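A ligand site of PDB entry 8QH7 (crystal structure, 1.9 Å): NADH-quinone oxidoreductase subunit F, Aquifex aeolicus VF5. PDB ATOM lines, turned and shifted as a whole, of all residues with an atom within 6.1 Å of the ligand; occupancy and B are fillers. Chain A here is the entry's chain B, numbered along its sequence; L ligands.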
ATOM      1  N   ILE A 181     -20.936  -2.677 -13.655  1.00  0.00           N
ATOM      2  CA  ILE A 181     -21.769  -2.388 -12.502  1.00  0.00           C
ATOM      3  C   ILE A 181     -23.087  -3.151 -12.602  1.00  0.00           C
ATOM      4  O   ILE A 181     -23.738  -3.324 -11.588  1.00  0.00           O
ATOM      5  CB  ILE A 181     -22.002  -0.872 -12.372  1.00  0.00           C
ATOM      6  CG1 ILE A 181     -22.622  -0.509 -11.029  1.00  0.00           C
ATOM      7  CG2 ILE A 181     -22.815  -0.326 -13.525  1.00  0.00           C
ATOM      8  CD1 ILE A 181     -21.836  -0.951  -9.836  1.00  0.00           C
ATOM      9  N   HIS A 198     -27.950   1.528 -12.397  1.00  0.00           N
ATOM     10  CA  HIS A 198     -27.668   2.307 -11.197  1.00  0.00           C
ATOM     11  C   HIS A 198     -28.051   1.481  -9.976  1.00  0.00           C
ATOM     12  O   HIS A 198     -29.249   1.205  -9.760  1.00  0.00           O
ATOM     13  CB  HIS A 198     -28.416   3.643 -11.266  1.00  0.00           C
ATOM     14  CG  HIS A 198     -27.823   4.628 -12.225  1.00  0.00           C
ATOM     15  ND1 HIS A 198     -28.458   5.801 -12.557  1.00  0.00           N
ATOM     16  CD2 HIS A 198     -26.665   4.637 -12.897  1.00  0.00           C
ATOM     17  CE1 HIS A 198     -27.683   6.502 -13.381  1.00  0.00           C
ATOM     18  NE2 HIS A 198     -26.600   5.804 -13.609  1.00  0.00           N
ATOM     19  N   PRO A 199     -27.075   1.072  -9.131  1.00  0.00           N
ATOM     20  CA  PRO A 199     -27.385   0.390  -7.871  1.00  0.00           C
ATOM     21  C   PRO A 199     -28.361   1.172  -6.992  1.00  0.00           C
ATOM     22  O   PRO A 199     -28.351   2.407  -6.984  1.00  0.00           O
ATOM     23  CB  PRO A 199     -26.021   0.253  -7.183  1.00  0.00           C
ATOM     24  CG  PRO A 199     -25.042   0.202  -8.347  1.00  0.00           C
ATOM     25  CD  PRO A 199     -25.624   1.173  -9.359  1.00  0.00           C
ATOM     26  N   GLU A 345     -15.570   2.015 -14.672  1.00  0.00           N
ATOM     27  CA  GLU A 345     -16.806   1.316 -14.330  1.00  0.00           C
ATOM     28  C   GLU A 345     -17.664   1.983 -13.245  1.00  0.00           C
ATOM     29  O   GLU A 345     -18.816   1.584 -13.076  1.00  0.00           O
ATOM     30  CB  GLU A 345     -16.502  -0.125 -13.941  1.00  0.00           C
ATOM     31  CG  GLU A 345     -15.814  -0.922 -15.037  1.00  0.00           C
ATOM     32  CD  GLU A 345     -16.535  -1.046 -16.360  1.00  0.00           C
ATOM     33  OE1 GLU A 345     -17.794  -0.903 -16.416  1.00  0.00           O
ATOM     34  OE2 GLU A 345     -15.848  -1.265 -17.373  1.00  0.00           O
ATOM     35  N   THR A 346     -17.171   2.999 -12.511  1.00  0.00           N
ATOM     36  CA  THR A 346     -18.057   3.693 -11.571  1.00  0.00           C
ATOM     37  C   THR A 346     -19.265   4.236 -12.322  1.00  0.00           C
ATOM     38  O   THR A 346     -19.123   4.832 -13.395  1.00  0.00           O
ATOM     39  CB  THR A 346     -17.346   4.805 -10.778  1.00  0.00           C
ATOM     40  OG1 THR A 346     -18.327   5.549 -10.032  1.00  0.00           O
ATOM     41  CG2 THR A 346     -16.572   5.766 -11.651  1.00  0.00           C
ATOM     42  N   CYS A 347     -20.452   4.066 -11.749  1.00  0.00           N
ATOM     43  CA  CYS A 347     -21.673   4.585 -12.360  1.00  0.00           C
ATOM     44  C   CYS A 347     -21.888   6.085 -12.081  1.00  0.00           C
ATOM     45  O   CYS A 347     -22.714   6.714 -12.743  1.00  0.00           O
ATOM     46  CB  CYS A 347     -22.885   3.758 -11.918  1.00  0.00           C
ATOM     47  SG  CYS A 347     -23.552   4.192 -10.282  1.00  0.00           S
ATOM     48  N   GLY A 348     -21.164   6.653 -11.093  1.00  0.00           N
ATOM     49  CA  GLY A 348     -21.133   8.092 -10.870  1.00  0.00           C
ATOM     50  C   GLY A 348     -22.233   8.663  -9.966  1.00  0.00           C
ATOM     51  O   GLY A 348     -22.279   9.870  -9.761  1.00  0.00           O
ATOM     52  N   GLN A 349     -23.118   7.815  -9.414  1.00  0.00           N
ATOM     53  CA  GLN A 349     -24.212   8.275  -8.560  1.00  0.00           C
ATOM     54  C   GLN A 349     -23.696   8.917  -7.279  1.00  0.00           C
ATOM     55  O   GLN A 349     -24.298   9.871  -6.777  1.00  0.00           O
ATOM     56  CB  GLN A 349     -25.102   7.116  -8.086  1.00  0.00           C
ATOM     57  CG  GLN A 349     -26.148   6.631  -9.064  1.00  0.00           C
ATOM     58  CD  GLN A 349     -27.038   5.671  -8.311  1.00  0.00           C
ATOM     59  OE1 GLN A 349     -28.080   6.088  -7.785  1.00  0.00           O
ATOM     60  NE2 GLN A 349     -26.572   4.437  -8.140  1.00  0.00           N
ATOM     61  N   CYS A 350     -22.620   8.338  -6.707  1.00  0.00           N
ATOM     62  CA  CYS A 350     -22.062   8.787  -5.438  1.00  0.00           C
ATOM     63  C   CYS A 350     -20.812   9.627  -5.726  1.00  0.00           C
ATOM     64  O   CYS A 350     -19.975   9.230  -6.532  1.00  0.00           O
ATOM     65  CB  CYS A 350     -21.709   7.615  -4.520  1.00  0.00           C
ATOM     66  SG  CYS A 350     -22.895   6.231  -4.533  1.00  0.00           S
ATOM     67  N   THR A 351     -20.691  10.787  -5.054  1.00  0.00           N
ATOM     68  CA  THR A 351     -19.673  11.759  -5.404  1.00  0.00           C
ATOM     69  C   THR A 351     -18.269  11.227  -5.121  1.00  0.00           C
ATOM     70  O   THR A 351     -17.409  11.312  -5.997  1.00  0.00           O
ATOM     71  CB  THR A 351     -19.942  13.129  -4.767  1.00  0.00           C
ATOM     72  OG1 THR A 351     -21.054  13.678  -5.466  1.00  0.00           O
ATOM     73  CG2 THR A 351     -18.756  14.074  -4.812  1.00  0.00           C
ATOM     74  N   CYS A 353     -17.085   8.186  -4.933  1.00  0.00           N
ATOM     75  CA  CYS A 353     -16.810   7.126  -5.899  1.00  0.00           C
ATOM     76  C   CYS A 353     -16.533   7.725  -7.278  1.00  0.00           C
ATOM     77  O   CYS A 353     -15.527   7.389  -7.925  1.00  0.00           O
ATOM     78  CB  CYS A 353     -17.961   6.131  -5.985  1.00  0.00           C
ATOM     79  SG  CYS A 353     -17.704   4.689  -7.075  1.00  0.00           S
ATOM     80  N   ARG A 354     -17.427   8.627  -7.709  1.00  0.00           N
ATOM     81  CA  ARG A 354     -17.335   9.254  -9.027  1.00  0.00           C
ATOM     82  C   ARG A 354     -15.979   9.942  -9.210  1.00  0.00           C
ATOM     83  O   ARG A 354     -15.238   9.617 -10.132  1.00  0.00           O
ATOM     84  CB  ARG A 354     -18.470  10.268  -9.191  1.00  0.00           C
ATOM     85  CG  ARG A 354     -18.474  10.995 -10.534  1.00  0.00           C
ATOM     86  CD  ARG A 354     -19.658  11.935 -10.690  1.00  0.00           C
ATOM     87  NE  ARG A 354     -19.673  13.037  -9.736  1.00  0.00           N
ATOM     88  CZ  ARG A 354     -20.565  13.185  -8.757  1.00  0.00           C
ATOM     89  NH1 ARG A 354     -21.422  12.221  -8.487  1.00  0.00           N
ATOM     90  NH2 ARG A 354     -20.558  14.293  -8.033  1.00  0.00           N
ATOM     91  N   CYS A 357     -12.676   7.444  -8.163  1.00  0.00           N
ATOM     92  CA  CYS A 357     -12.220   6.442  -9.126  1.00  0.00           C
ATOM     93  C   CYS A 357     -11.451   7.127 -10.255  1.00  0.00           C
ATOM     94  O   CYS A 357     -10.394   6.658 -10.661  1.00  0.00           O
ATOM     95  CB  CYS A 357     -13.370   5.605  -9.681  1.00  0.00           C
ATOM     96  SG  CYS A 357     -14.019   4.433  -8.462  1.00  0.00           S
ATOM     97  N   THR A 390     -19.958   7.487   1.721  1.00  0.00           N
ATOM     98  CA  THR A 390     -21.288   7.664   1.163  1.00  0.00           C
ATOM     99  C   THR A 390     -21.654   6.655   0.062  1.00  0.00           C
ATOM    100  O   THR A 390     -22.784   6.724  -0.445  1.00  0.00           O
ATOM    101  CB  THR A 390     -21.527   9.087   0.636  1.00  0.00           C
ATOM    102  OG1 THR A 390     -21.004   9.205  -0.687  1.00  0.00           O
ATOM    103  CG2 THR A 390     -20.935  10.156   1.527  1.00  0.00           C
ATOM    104  N   SER A 391     -20.755   5.716  -0.308  1.00  0.00           N
ATOM    105  CA  SER A 391     -21.031   4.784  -1.391  1.00  0.00           C
ATOM    106  C   SER A 391     -22.259   3.910  -1.093  1.00  0.00           C
ATOM    107  O   SER A 391     -22.457   3.495   0.042  1.00  0.00           O
ATOM    108  CB  SER A 391     -19.821   3.932  -1.673  1.00  0.00           C
ATOM    109  OG  SER A 391     -19.446   3.214  -0.508  1.00  0.00           O
ATOM    110  N   ILE A 392     -23.072   3.619  -2.114  1.00  0.00           N
ATOM    111  CA  ILE A 392     -24.241   2.778  -1.909  1.00  0.00           C
ATOM    112  C   ILE A 392     -24.047   1.381  -2.514  1.00  0.00           C
ATOM    113  O   ILE A 392     -25.010   0.607  -2.505  1.00  0.00           O
ATOM    114  CB  ILE A 392     -25.542   3.436  -2.413  1.00  0.00           C
ATOM    115  CG1 ILE A 392     -25.547   3.720  -3.919  1.00  0.00           C
ATOM    116  CG2 ILE A 392     -25.819   4.679  -1.598  1.00  0.00           C
ATOM    117  CD1 ILE A 392     -26.845   4.350  -4.398  1.00  0.00           C
ATOM    118  N   CYS A 393     -22.852   1.055  -3.004  1.00  0.00           N
ATOM    119  CA  CYS A 393     -22.615  -0.298  -3.499  1.00  0.00           C
ATOM    120  C   CYS A 393     -21.145  -0.644  -3.302  1.00  0.00           C
ATOM    121  O   CYS A 393     -20.329   0.211  -2.929  1.00  0.00           O
ATOM    122  CB  CYS A 393     -23.059  -0.517  -4.953  1.00  0.00           C
ATOM    123  SG  CYS A 393     -21.796  -0.245  -6.226  1.00  0.00           S
ATOM    124  N   GLY A 394     -20.840  -1.917  -3.546  1.00  0.00           N
ATOM    125  CA  GLY A 394     -19.560  -2.492  -3.206  1.00  0.00           C
ATOM    126  C   GLY A 394     -18.401  -1.965  -4.050  1.00  0.00           C
ATOM    127  O   GLY A 394     -17.261  -2.152  -3.647  1.00  0.00           O
ATOM    128  N   LEU A 395     -18.683  -1.342  -5.208  1.00  0.00           N
ATOM    129  CA  LEU A 395     -17.618  -0.849  -6.079  1.00  0.00           C
ATOM    130  C   LEU A 395     -16.867   0.273  -5.371  1.00  0.00           C
ATOM    131  O   LEU A 395     -15.638   0.207  -5.209  1.00  0.00           O
ATOM    132  CB  LEU A 395     -18.220  -0.394  -7.416  1.00  0.00           C
ATOM    133  CG  LEU A 395     -17.211  -0.098  -8.527  1.00  0.00           C
ATOM    134  CD1 LEU A 395     -17.848  -0.241  -9.907  1.00  0.00           C
ATOM    135  CD2 LEU A 395     -16.602   1.309  -8.374  1.00  0.00           C
ATOM    136  N   GLY A 396     -17.604   1.288  -4.899  1.00  0.00           N
ATOM    137  CA  GLY A 396     -17.000   2.384  -4.159  1.00  0.00           C
ATOM    138  C   GLY A 396     -16.333   1.899  -2.869  1.00  0.00           C
ATOM    139  O   GLY A 396     -15.295   2.423  -2.461  1.00  0.00           O
ATOM    140  N   ALA A 397     -16.915   0.866  -2.256  1.00  0.00           N
ATOM    141  CA  ALA A 397     -16.364   0.304  -1.022  1.00  0.00           C
ATOM    142  C   ALA A 397     -14.961  -0.275  -1.250  1.00  0.00           C
ATOM    143  O   ALA A 397     -14.173  -0.292  -0.314  1.00  0.00           O
ATOM    144  CB  ALA A 397     -17.296  -0.732  -0.460  1.00  0.00           C
HETATM  145 FE1  LIG L   1     -22.188   3.854  -8.543  1.00  0.00          FE
HETATM  146 FE2  LIG L   1     -19.793   3.915  -7.133  1.00  0.00          FE
HETATM  147 FE3  LIG L   1     -21.644   1.999  -6.553  1.00  0.00          FE
HETATM  148 FE4  LIG L   1     -22.097   4.649  -5.913  1.00  0.00          FE
HETATM  149  S1  LIG L   1     -20.456   3.245  -5.038  1.00  0.00           S
HETATM  150  S2  LIG L   1     -23.630   3.193  -6.815  1.00  0.00           S
HETATM  151  S3  LIG L   1     -21.125   5.697  -7.724  1.00  0.00           S
HETATM  152  S4  LIG L   1     -20.518   2.277  -8.545  1.00  0.00           S
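A sulfur (S3) of the ligand lies close to the backbone NH of Gln 349 (3.4 Å). The side-chain sulfur of Cys 350 is bound to an iron atom (FE4) of the ligand (2.2 Å). S4 of the ligand sits close to N of Cys 347 (3.7 Å). S3 of the ligand sits close to N of Gly 348. The backbone NH (N) of Cys 350 lies close to a sulfur (S3) of the ligand, 3.2 Å away. The backbone NH (N) of Gly 396 lies close to a sulfur (S1) of the ligand (3.5 Å). FE2 of the ligand is bound by SG of Cys 353. A sulfur (S3) of the ligand sits close to the side-chain hydroxyl (OG1) of Thr 346 (3.6 Å). S2 of the ligand lies close to NE2 of Gln 349 (3.5 Å). The side-chain sulfur (SG) of Cys 393 is bound to an iron atom (FE3) of the ligand, at 2.3 Å. The side-chain sulfur (SG) of Cys 347 binds an iron atom (FE1) of the ligand.
The backbone carbonyl oxygen of Pro 199 is in hydrogen-bond range of the side-chain amide nitrogen of Gln 349, 2.9 Å away. SG of Cys 353 lies close to OG1 of Thr 346, at 3.1 Å. SG of Cys 347 sits close to NE2 of Gln 349 (3.7 Å). N of Leu 395 lies close to SG of Cys 393, 3.5 Å away. The backbone NH (N) of Gly 348 sits at hydrogen-bond distance from the side-chain hydroxyl (OG1) of Thr 346. O of Gly 348 lies within hydrogen-bond range of NH1 of Arg 354. The side-chain sulfur (SG) of Cys 350 lies close to the backbone NH (N) of Ile 392, 3.6 Å away. SG of Cys 357 sits close to O of Cys 353 (3.4 Å).
Residues that only touch the ligand: Ser 391 (3.5 Å), Ile 392 (3.5 Å), Pro 199 (3.6 Å), Leu 395 (3.7 Å) and Ile 181 (3.7 Å). Hydrophobic or aromatic side chains that line the ligand: Ile 181, Pro 199, Ile 392 and Leu 395. 13 residues have an atom within 4 Å of the ligand: Ile 181, Pro 199, Thr 346, Cys 347, Gly 348, Gln 349, Cys 350, Cys 353, Ser 391, Ile 392, Cys 393, Leu 395 and Gly 396.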
